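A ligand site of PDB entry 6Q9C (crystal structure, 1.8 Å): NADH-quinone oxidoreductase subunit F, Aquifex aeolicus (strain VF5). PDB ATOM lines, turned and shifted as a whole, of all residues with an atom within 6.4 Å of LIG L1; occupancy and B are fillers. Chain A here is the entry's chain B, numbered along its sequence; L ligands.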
ATOM      1  N   ILE A 180      18.686 -14.285 -15.165  1.00  0.00           N
ATOM      2  CA  ILE A 180      18.030 -15.195 -16.158  1.00  0.00           C
ATOM      3  C   ILE A 180      19.020 -15.520 -17.292  1.00  0.00           C
ATOM      4  O   ILE A 180      18.820 -16.553 -17.920  1.00  0.00           O
ATOM      5  CB  ILE A 180      16.707 -14.596 -16.677  1.00  0.00           C
ATOM      6  CG1 ILE A 180      15.858 -15.646 -17.396  1.00  0.00           C
ATOM      7  CG2 ILE A 180      16.955 -13.391 -17.568  1.00  0.00           C
ATOM      8  CD1 ILE A 180      15.623 -16.895 -16.578  1.00  0.00           C
ATOM      9  N   GLU A 183      20.388 -18.955 -17.442  1.00  0.00           N
ATOM     10  CA  GLU A 183      19.569 -20.021 -18.062  1.00  0.00           C
ATOM     11  C   GLU A 183      20.118 -20.228 -19.475  1.00  0.00           C
ATOM     12  O   GLU A 183      20.293 -19.221 -20.198  1.00  0.00           O
ATOM     13  CB  GLU A 183      18.082 -19.646 -18.013  1.00  0.00           C
ATOM     14  CG  GLU A 183      17.138 -20.828 -18.189  1.00  0.00           C
ATOM     15  CD  GLU A 183      16.882 -21.281 -19.624  1.00  0.00           C
ATOM     16  OE1 GLU A 183      17.333 -20.604 -20.589  1.00  0.00           O
ATOM     17  OE2 GLU A 183      16.202 -22.313 -19.768  1.00  0.00           O
ATOM     18  N   GLY A 196      17.773 -11.427 -22.732  1.00  0.00           N
ATOM     19  CA  GLY A 196      17.868 -12.778 -22.135  1.00  0.00           C
ATOM     20  C   GLY A 196      16.488 -13.379 -21.870  1.00  0.00           C
ATOM     21  O   GLY A 196      16.057 -13.416 -20.696  1.00  0.00           O
ATOM     22  N   HIS A 197      15.805 -13.788 -22.933  1.00  0.00           N
ATOM     23  CA  HIS A 197      14.484 -14.476 -22.880  1.00  0.00           C
ATOM     24  C   HIS A 197      14.700 -15.957 -23.156  1.00  0.00           C
ATOM     25  O   HIS A 197      15.055 -16.331 -24.271  1.00  0.00           O
ATOM     26  CB  HIS A 197      13.506 -13.817 -23.863  1.00  0.00           C
ATOM     27  CG  HIS A 197      13.022 -12.479 -23.416  1.00  0.00           C
ATOM     28  ND1 HIS A 197      12.274 -11.664 -24.239  1.00  0.00           N
ATOM     29  CD2 HIS A 197      13.178 -11.803 -22.260  1.00  0.00           C
ATOM     30  CE1 HIS A 197      11.965 -10.558 -23.593  1.00  0.00           C
ATOM     31  NE2 HIS A 197      12.514 -10.606 -22.389  1.00  0.00           N
ATOM     32  N   PRO A 198      14.534 -16.833 -22.137  1.00  0.00           N
ATOM     33  CA  PRO A 198      14.594 -18.273 -22.360  1.00  0.00           C
ATOM     34  C   PRO A 198      13.693 -18.736 -23.506  1.00  0.00           C
ATOM     35  O   PRO A 198      12.671 -18.096 -23.784  1.00  0.00           O
ATOM     36  CB  PRO A 198      14.125 -18.862 -21.013  1.00  0.00           C
ATOM     37  CG  PRO A 198      14.521 -17.802 -19.992  1.00  0.00           C
ATOM     38  CD  PRO A 198      14.349 -16.477 -20.718  1.00  0.00           C
ATOM     39  N   ARG A 199      14.096 -19.818 -24.173  1.00  0.00           N
ATOM     40  CA  ARG A 199      13.353 -20.458 -25.286  1.00  0.00           C
ATOM     41  C   ARG A 199      12.592 -21.669 -24.744  1.00  0.00           C
ATOM     42  O   ARG A 199      13.117 -22.346 -23.834  1.00  0.00           O
ATOM     43  CB  ARG A 199      14.319 -20.929 -26.377  1.00  0.00           C
ATOM     44  CG  ARG A 199      15.193 -19.839 -26.964  1.00  0.00           C
ATOM     45  CD  ARG A 199      16.223 -20.491 -27.861  1.00  0.00           C
ATOM     46  NE  ARG A 199      17.054 -19.531 -28.564  1.00  0.00           N
ATOM     47  CZ  ARG A 199      18.049 -19.859 -29.389  1.00  0.00           C
ATOM     48  NH1 ARG A 199      18.751 -18.909 -29.976  1.00  0.00           N
ATOM     49  NH2 ARG A 199      18.331 -21.132 -29.620  1.00  0.00           N
ATOM     50  N   GLU A 344      14.193 -10.836 -10.833  1.00  0.00           N
ATOM     51  CA  GLU A 344      14.891 -11.576 -11.926  1.00  0.00           C
ATOM     52  C   GLU A 344      13.937 -12.226 -12.935  1.00  0.00           C
ATOM     53  O   GLU A 344      14.419 -12.569 -14.016  1.00  0.00           O
ATOM     54  CB  GLU A 344      15.844 -12.603 -11.314  1.00  0.00           C
ATOM     55  CG  GLU A 344      16.917 -11.964 -10.451  1.00  0.00           C
ATOM     56  CD  GLU A 344      17.794 -10.904 -11.093  1.00  0.00           C
ATOM     57  OE1 GLU A 344      17.895 -10.858 -12.347  1.00  0.00           O
ATOM     58  OE2 GLU A 344      18.413 -10.139 -10.327  1.00  0.00           O
ATOM     59  N   THR A 345      12.643 -12.400 -12.660  1.00  0.00           N
ATOM     60  CA  THR A 345      11.718 -12.956 -13.691  1.00  0.00           C
ATOM     61  C   THR A 345      11.810 -12.103 -14.963  1.00  0.00           C
ATOM     62  O   THR A 345      11.827 -10.856 -14.849  1.00  0.00           O
ATOM     63  CB  THR A 345      10.263 -13.065 -13.194  1.00  0.00           C
ATOM     64  OG1 THR A 345       9.512 -13.505 -14.322  1.00  0.00           O
ATOM     65  CG2 THR A 345       9.708 -11.767 -12.648  1.00  0.00           C
ATOM     66  N   CYS A 346      11.881 -12.731 -16.146  1.00  0.00           N
ATOM     67  CA  CYS A 346      11.994 -12.025 -17.451  1.00  0.00           C
ATOM     68  C   CYS A 346      10.604 -11.580 -17.933  1.00  0.00           C
ATOM     69  O   CYS A 346      10.549 -10.673 -18.795  1.00  0.00           O
ATOM     70  CB  CYS A 346      12.742 -12.856 -18.491  1.00  0.00           C
ATOM     71  SG  CYS A 346      11.734 -14.133 -19.286  1.00  0.00           S
ATOM     72  N   GLY A 347       9.532 -12.181 -17.409  1.00  0.00           N
ATOM     73  CA  GLY A 347       8.143 -11.719 -17.596  1.00  0.00           C
ATOM     74  C   GLY A 347       7.446 -12.302 -18.815  1.00  0.00           C
ATOM     75  O   GLY A 347       6.297 -11.896 -19.071  1.00  0.00           O
ATOM     76  N   GLN A 348       8.082 -13.218 -19.549  1.00  0.00           N
ATOM     77  CA  GLN A 348       7.496 -13.853 -20.763  1.00  0.00           C
ATOM     78  C   GLN A 348       6.230 -14.631 -20.400  1.00  0.00           C
ATOM     79  O   GLN A 348       5.272 -14.612 -21.197  1.00  0.00           O
ATOM     80  CB  GLN A 348       8.456 -14.868 -21.393  1.00  0.00           C
ATOM     81  CG  GLN A 348       9.490 -14.269 -22.332  1.00  0.00           C
ATOM     82  CD  GLN A 348      10.145 -15.384 -23.100  1.00  0.00           C
ATOM     83  OE1 GLN A 348       9.815 -15.632 -24.253  1.00  0.00           O
ATOM     84  NE2 GLN A 348      11.040 -16.103 -22.427  1.00  0.00           N
ATOM     85  N   CYS A 349       6.265 -15.339 -19.268  1.00  0.00           N
ATOM     86  CA  CYS A 349       5.162 -16.222 -18.802  1.00  0.00           C
ATOM     87  C   CYS A 349       4.333 -15.491 -17.746  1.00  0.00           C
ATOM     88  O   CYS A 349       4.920 -14.878 -16.845  1.00  0.00           O
ATOM     89  CB  CYS A 349       5.696 -17.536 -18.251  1.00  0.00           C
ATOM     90  SG  CYS A 349       7.092 -18.194 -19.208  1.00  0.00           S
ATOM     91  N   THR A 350       3.010 -15.530 -17.857  1.00  0.00           N
ATOM     92  CA  THR A 350       2.134 -14.688 -17.012  1.00  0.00           C
ATOM     93  C   THR A 350       2.228 -15.128 -15.549  1.00  0.00           C
ATOM     94  O   THR A 350       2.452 -14.281 -14.689  1.00  0.00           O
ATOM     95  CB  THR A 350       0.711 -14.633 -17.575  1.00  0.00           C
ATOM     96  OG1 THR A 350       0.803 -13.842 -18.764  1.00  0.00           O
ATOM     97  CG2 THR A 350      -0.286 -14.014 -16.616  1.00  0.00           C
ATOM     98  N   CYS A 352       4.504 -16.597 -13.870  1.00  0.00           N
ATOM     99  CA  CYS A 352       5.865 -16.244 -13.367  1.00  0.00           C
ATOM    100  C   CYS A 352       5.971 -14.721 -13.185  1.00  0.00           C
ATOM    101  O   CYS A 352       6.373 -14.281 -12.097  1.00  0.00           O
ATOM    102  CB  CYS A 352       6.955 -16.759 -14.290  1.00  0.00           C
ATOM    103  SG  CYS A 352       8.619 -16.432 -13.646  1.00  0.00           S
ATOM    104  N   ARG A 353       5.585 -13.950 -14.205  1.00  0.00           N
ATOM    105  CA  ARG A 353       5.649 -12.468 -14.186  1.00  0.00           C
ATOM    106  C   ARG A 353       4.867 -11.929 -12.977  1.00  0.00           C
ATOM    107  O   ARG A 353       5.443 -11.148 -12.179  1.00  0.00           O
ATOM    108  CB  ARG A 353       5.075 -11.890 -15.476  1.00  0.00           C
ATOM    109  CG  ARG A 353       5.126 -10.363 -15.549  1.00  0.00           C
ATOM    110  CD  ARG A 353       4.636  -9.815 -16.882  1.00  0.00           C
ATOM    111  NE  ARG A 353       3.225 -10.087 -17.120  1.00  0.00           N
ATOM    112  CZ  ARG A 353       2.736 -11.047 -17.895  1.00  0.00           C
ATOM    113  NH1 ARG A 353       3.539 -11.892 -18.525  1.00  0.00           N
ATOM    114  NH2 ARG A 353       1.420 -11.153 -18.025  1.00  0.00           N
ATOM    115  N   CYS A 356       5.890 -13.918  -9.205  1.00  0.00           N
ATOM    116  CA  CYS A 356       7.173 -13.483  -8.563  1.00  0.00           C
ATOM    117  C   CYS A 356       6.967 -12.103  -7.920  1.00  0.00           C
ATOM    118  O   CYS A 356       7.396 -11.914  -6.764  1.00  0.00           O
ATOM    119  CB  CYS A 356       8.324 -13.460  -9.570  1.00  0.00           C
ATOM    120  SG  CYS A 356       8.880 -15.121 -10.002  1.00  0.00           S
ATOM    121  N   ILE A 386       3.104 -20.097  -9.282  1.00  0.00           N
ATOM    122  CA  ILE A 386       4.110 -19.371 -10.115  1.00  0.00           C
ATOM    123  C   ILE A 386       4.510 -20.240 -11.311  1.00  0.00           C
ATOM    124  O   ILE A 386       4.764 -19.680 -12.396  1.00  0.00           O
ATOM    125  CB  ILE A 386       5.328 -18.923  -9.279  1.00  0.00           C
ATOM    126  CG1 ILE A 386       4.896 -18.086  -8.072  1.00  0.00           C
ATOM    127  CG2 ILE A 386       6.308 -18.152 -10.143  1.00  0.00           C
ATOM    128  CD1 ILE A 386       5.991 -17.762  -7.089  1.00  0.00           C
ATOM    129  N   THR A 389       2.582 -22.968 -16.793  1.00  0.00           N
ATOM    130  CA  THR A 389       2.903 -22.475 -18.155  1.00  0.00           C
ATOM    131  C   THR A 389       4.359 -21.989 -18.256  1.00  0.00           C
ATOM    132  O   THR A 389       4.734 -21.593 -19.367  1.00  0.00           O
ATOM    133  CB  THR A 389       1.943 -21.364 -18.619  1.00  0.00           C
ATOM    134  OG1 THR A 389       2.338 -20.128 -18.018  1.00  0.00           O
ATOM    135  CG2 THR A 389       0.505 -21.670 -18.311  1.00  0.00           C
ATOM    136  N   SER A 390       5.149 -22.048 -17.179  1.00  0.00           N
ATOM    137  CA  SER A 390       6.560 -21.577 -17.170  1.00  0.00           C
ATOM    138  C   SER A 390       7.370 -22.316 -18.248  1.00  0.00           C
ATOM    139  O   SER A 390       7.143 -23.532 -18.429  1.00  0.00           O
ATOM    140  CB  SER A 390       7.177 -21.727 -15.805  1.00  0.00           C
ATOM    141  OG  SER A 390       7.105 -23.073 -15.367  1.00  0.00           O
ATOM    142  N   ILE A 391       8.277 -21.627 -18.944  1.00  0.00           N
ATOM    143  CA  ILE A 391       9.123 -22.259 -20.005  1.00  0.00           C
ATOM    144  C   ILE A 391      10.576 -22.345 -19.535  1.00  0.00           C
ATOM    145  O   ILE A 391      11.420 -22.796 -20.340  1.00  0.00           O
ATOM    146  CB  ILE A 391       8.984 -21.552 -21.367  1.00  0.00           C
ATOM    147  CG1 ILE A 391       9.474 -20.097 -21.365  1.00  0.00           C
ATOM    148  CG2 ILE A 391       7.542 -21.638 -21.857  1.00  0.00           C
ATOM    149  CD1 ILE A 391       9.537 -19.483 -22.754  1.00  0.00           C
ATOM    150  N   CYS A 392      10.886 -21.943 -18.289  1.00  0.00           N
ATOM    151  CA  CYS A 392      12.252 -22.140 -17.731  1.00  0.00           C
ATOM    152  C   CYS A 392      12.197 -22.439 -16.232  1.00  0.00           C
ATOM    153  O   CYS A 392      11.118 -22.315 -15.629  1.00  0.00           O
ATOM    154  CB  CYS A 392      13.175 -20.970 -18.078  1.00  0.00           C
ATOM    155  SG  CYS A 392      13.310 -19.688 -16.815  1.00  0.00           S
ATOM    156  N   GLY A 393      13.327 -22.876 -15.696  1.00  0.00           N
ATOM    157  CA  GLY A 393      13.496 -23.314 -14.294  1.00  0.00           C
ATOM    158  C   GLY A 393      13.171 -22.237 -13.267  1.00  0.00           C
ATOM    159  O   GLY A 393      12.906 -22.628 -12.120  1.00  0.00           O
ATOM    160  N   LEU A 394      13.215 -20.946 -13.628  1.00  0.00           N
ATOM    161  CA  LEU A 394      12.973 -19.838 -12.666  1.00  0.00           C
ATOM    162  C   LEU A 394      11.518 -19.918 -12.184  1.00  0.00           C
ATOM    163  O   LEU A 394      11.299 -20.040 -10.965  1.00  0.00           O
ATOM    164  CB  LEU A 394      13.286 -18.469 -13.289  1.00  0.00           C
ATOM    165  CG  LEU A 394      13.396 -17.309 -12.285  1.00  0.00           C
ATOM    166  CD1 LEU A 394      14.379 -16.246 -12.759  1.00  0.00           C
ATOM    167  CD2 LEU A 394      12.038 -16.679 -12.015  1.00  0.00           C
ATOM    168  N   GLY A 395      10.564 -19.855 -13.111  1.00  0.00           N
ATOM    169  CA  GLY A 395       9.130 -20.040 -12.824  1.00  0.00           C
ATOM    170  C   GLY A 395       8.891 -21.336 -12.049  1.00  0.00           C
ATOM    171  O   GLY A 395       8.086 -21.316 -11.092  1.00  0.00           O
ATOM    172  N   ALA A 396       9.576 -22.418 -12.430  1.00  0.00           N
ATOM    173  CA  ALA A 396       9.396 -23.763 -11.812  1.00  0.00           C
ATOM    174  C   ALA A 396       9.769 -23.755 -10.325  1.00  0.00           C
ATOM    175  O   ALA A 396       9.172 -24.558  -9.595  1.00  0.00           O
ATOM    176  CB  ALA A 396      10.180 -24.789 -12.588  1.00  0.00           C
HETATM  177 FE1  LIG L   1      10.914 -15.770 -17.900  1.00  0.00          FE
HETATM  178 FE2  LIG L   1       9.780 -16.821 -15.605  1.00  0.00          FE
HETATM  179 FE3  LIG L   1      11.491 -18.320 -17.098  1.00  0.00          FE
HETATM  180 FE4  LIG L   1       9.009 -17.706 -18.074  1.00  0.00          FE
HETATM  181  S1  LIG L   1       9.505 -18.995 -16.231  1.00  0.00           S
HETATM  182  S2  LIG L   1      10.967 -17.627 -19.221  1.00  0.00           S
HETATM  183  S3  LIG L   1       8.720 -15.589 -17.263  1.00  0.00           S
HETATM  184  S4  LIG L   1      11.990 -16.374 -15.970  1.00  0.00           S
HETATM  185  N1  LG2 L   2      24.060 -22.663 -14.981  1.00  0.00           N
HETATM  186  C1  LG2 L   2      25.305 -22.144 -14.810  1.00  0.00           C
HETATM  187  O1  LG2 L   2      26.323 -22.777 -15.117  1.00  0.00           O
HETATM  188  N2  LG2 L   2      25.447 -20.844 -14.338  1.00  0.00           N
HETATM  189  C2  LG2 L   2      24.411 -19.967 -14.045  1.00  0.00           C
HETATM  190  O2  LG2 L   2      24.648 -18.844 -13.601  1.00  0.00           O
HETATM  191  C3  LG2 L   2      23.084 -20.524 -14.282  1.00  0.00           C
HETATM  192  N3  LG2 L   2      22.048 -19.754 -14.083  1.00  0.00           N
HETATM  193  C4  LG2 L   2      20.790 -20.289 -14.324  1.00  0.00           C
HETATM  194  C5  LG2 L   2      19.658 -19.480 -14.115  1.00  0.00           C
HETATM  195  C6  LG2 L   2      18.372 -19.988 -14.283  1.00  0.00           C
HETATM  196  C7  LG2 L   2      17.186 -19.091 -14.004  1.00  0.00           C
HETATM  197  C8  LG2 L   2      18.207 -21.324 -14.680  1.00  0.00           C
HETATM  198  C9  LG2 L   2      16.835 -21.938 -14.812  1.00  0.00           C
HETATM  199  C10 LG2 L   2      19.317 -22.120 -14.916  1.00  0.00           C
HETATM  200  C11 LG2 L   2      20.607 -21.623 -14.734  1.00  0.00           C
HETATM  201  N4  LG2 L   2      21.764 -22.418 -14.943  1.00  0.00           N
HETATM  202  C12 LG2 L   2      23.014 -21.894 -14.731  1.00  0.00           C
HETATM  203  C13 LG2 L   2      21.671 -23.782 -15.478  1.00  0.00           C
HETATM  204  C14 LG2 L   2      21.871 -23.818 -16.981  1.00  0.00           C
HETATM  205  O3  LG2 L   2      20.636 -23.570 -17.663  1.00  0.00           O
HETATM  206  C15 LG2 L   2      22.444 -25.153 -17.446  1.00  0.00           C
HETATM  207  O4  LG2 L   2      21.719 -26.245 -16.879  1.00  0.00           O
HETATM  208  C16 LG2 L   2      23.921 -25.382 -17.133  1.00  0.00           C
HETATM  209  O5  LG2 L   2      24.687 -24.225 -17.439  1.00  0.00           O
HETATM  210  C17 LG2 L   2      24.417 -26.590 -17.908  1.00  0.00           C
HETATM  211  O6  LG2 L   2      25.783 -26.872 -17.519  1.00  0.00           O
HETATM  212  P1  LG2 L   2      26.103 -28.140 -16.608  1.00  0.00           P
HETATM  213  O7  LG2 L   2      25.638 -27.925 -15.184  1.00  0.00           O
HETATM  214  O8  LG2 L   2      25.432 -29.335 -17.245  1.00  0.00           O
HETATM  215  O9  LG2 L   2      27.637 -28.296 -16.719  1.00  0.00           O
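Merely in contact with LIG L1: Ile 391 (3.6 Å), Ser 390 (3.6 Å), Pro 198 (3.6 Å), Leu 394 (3.6 Å) and Ile 180 (3.7 Å). Hydrophobic or aromatic side chains within 4 Å of LIG L1: Ile 180, Pro 198, Ile 391 and Leu 394. Of the 25 residues printed, 13 come within 4 Å of LIG L1. The nearest printed residue that does not touch LIG L1 is Arg 353 (4.7 Å).
N of Cys 349 lies close to S3 of LIG L1 (3.2 Å). SG of Cys 349 is bound to FE4 of LIG L1 (2.3 Å). FE3 of LIG L1 is bound by SG of Cys 392 (2.3 Å). The backbone NH (N) of Cys 346 lies close to a sulfur (S4) of LIG L1 (3.6 Å). The side-chain sulfur (SG) of Cys 346 is bound to an iron atom (FE1) of LIG L1 (2.3 Å). An iron atom (FE2) of LIG L1 is bound by the side-chain sulfur (SG) of Cys 352 (2.3 Å). The backbone NH (N) of Gln 348 lies close to a sulfur (S3) of LIG L1 (3.4 Å). S2 of LIG L1 sits close to NE2 of Gln 348 (3.6 Å). N of Gly 395 lies close to S1 of LIG L1 (3.4 Å). The backbone NH (N) of Gly 347 lies close to a sulfur (S3) of LIG L1. OG1 of Thr 345 sits close to S3 of LIG L1 (3.7 Å).
SG of Cys 349 sits close to N of Ile 391 (3.6 Å). SG of Cys 392 sits close to N of Leu 394, 3.4 Å away. The side-chain sulfur (SG) of Cys 352 lies close to the side-chain hydroxyl (OG1) of Thr 345, at 3.1 Å. The side-chain sulfur of Cys 356 lies close to the backbone carbonyl oxygen of Cys 352, 3.4 Å away. The backbone NH (N) of Cys 352 lies within hydrogen-bond range of the backbone carbonyl oxygen (O) of Ile 386, at 3.4 Å. NE2 of Gln 348 is in hydrogen-bond range of O of Pro 198, at 2.9 Å. The side-chain hydroxyl (OG1) of Thr 345 sits close to the backbone NH (N) of Gly 347, at 3.4 Å. O of Gly 347 is in hydrogen-bond range of NH1 of Arg 353, at 2.8 Å.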
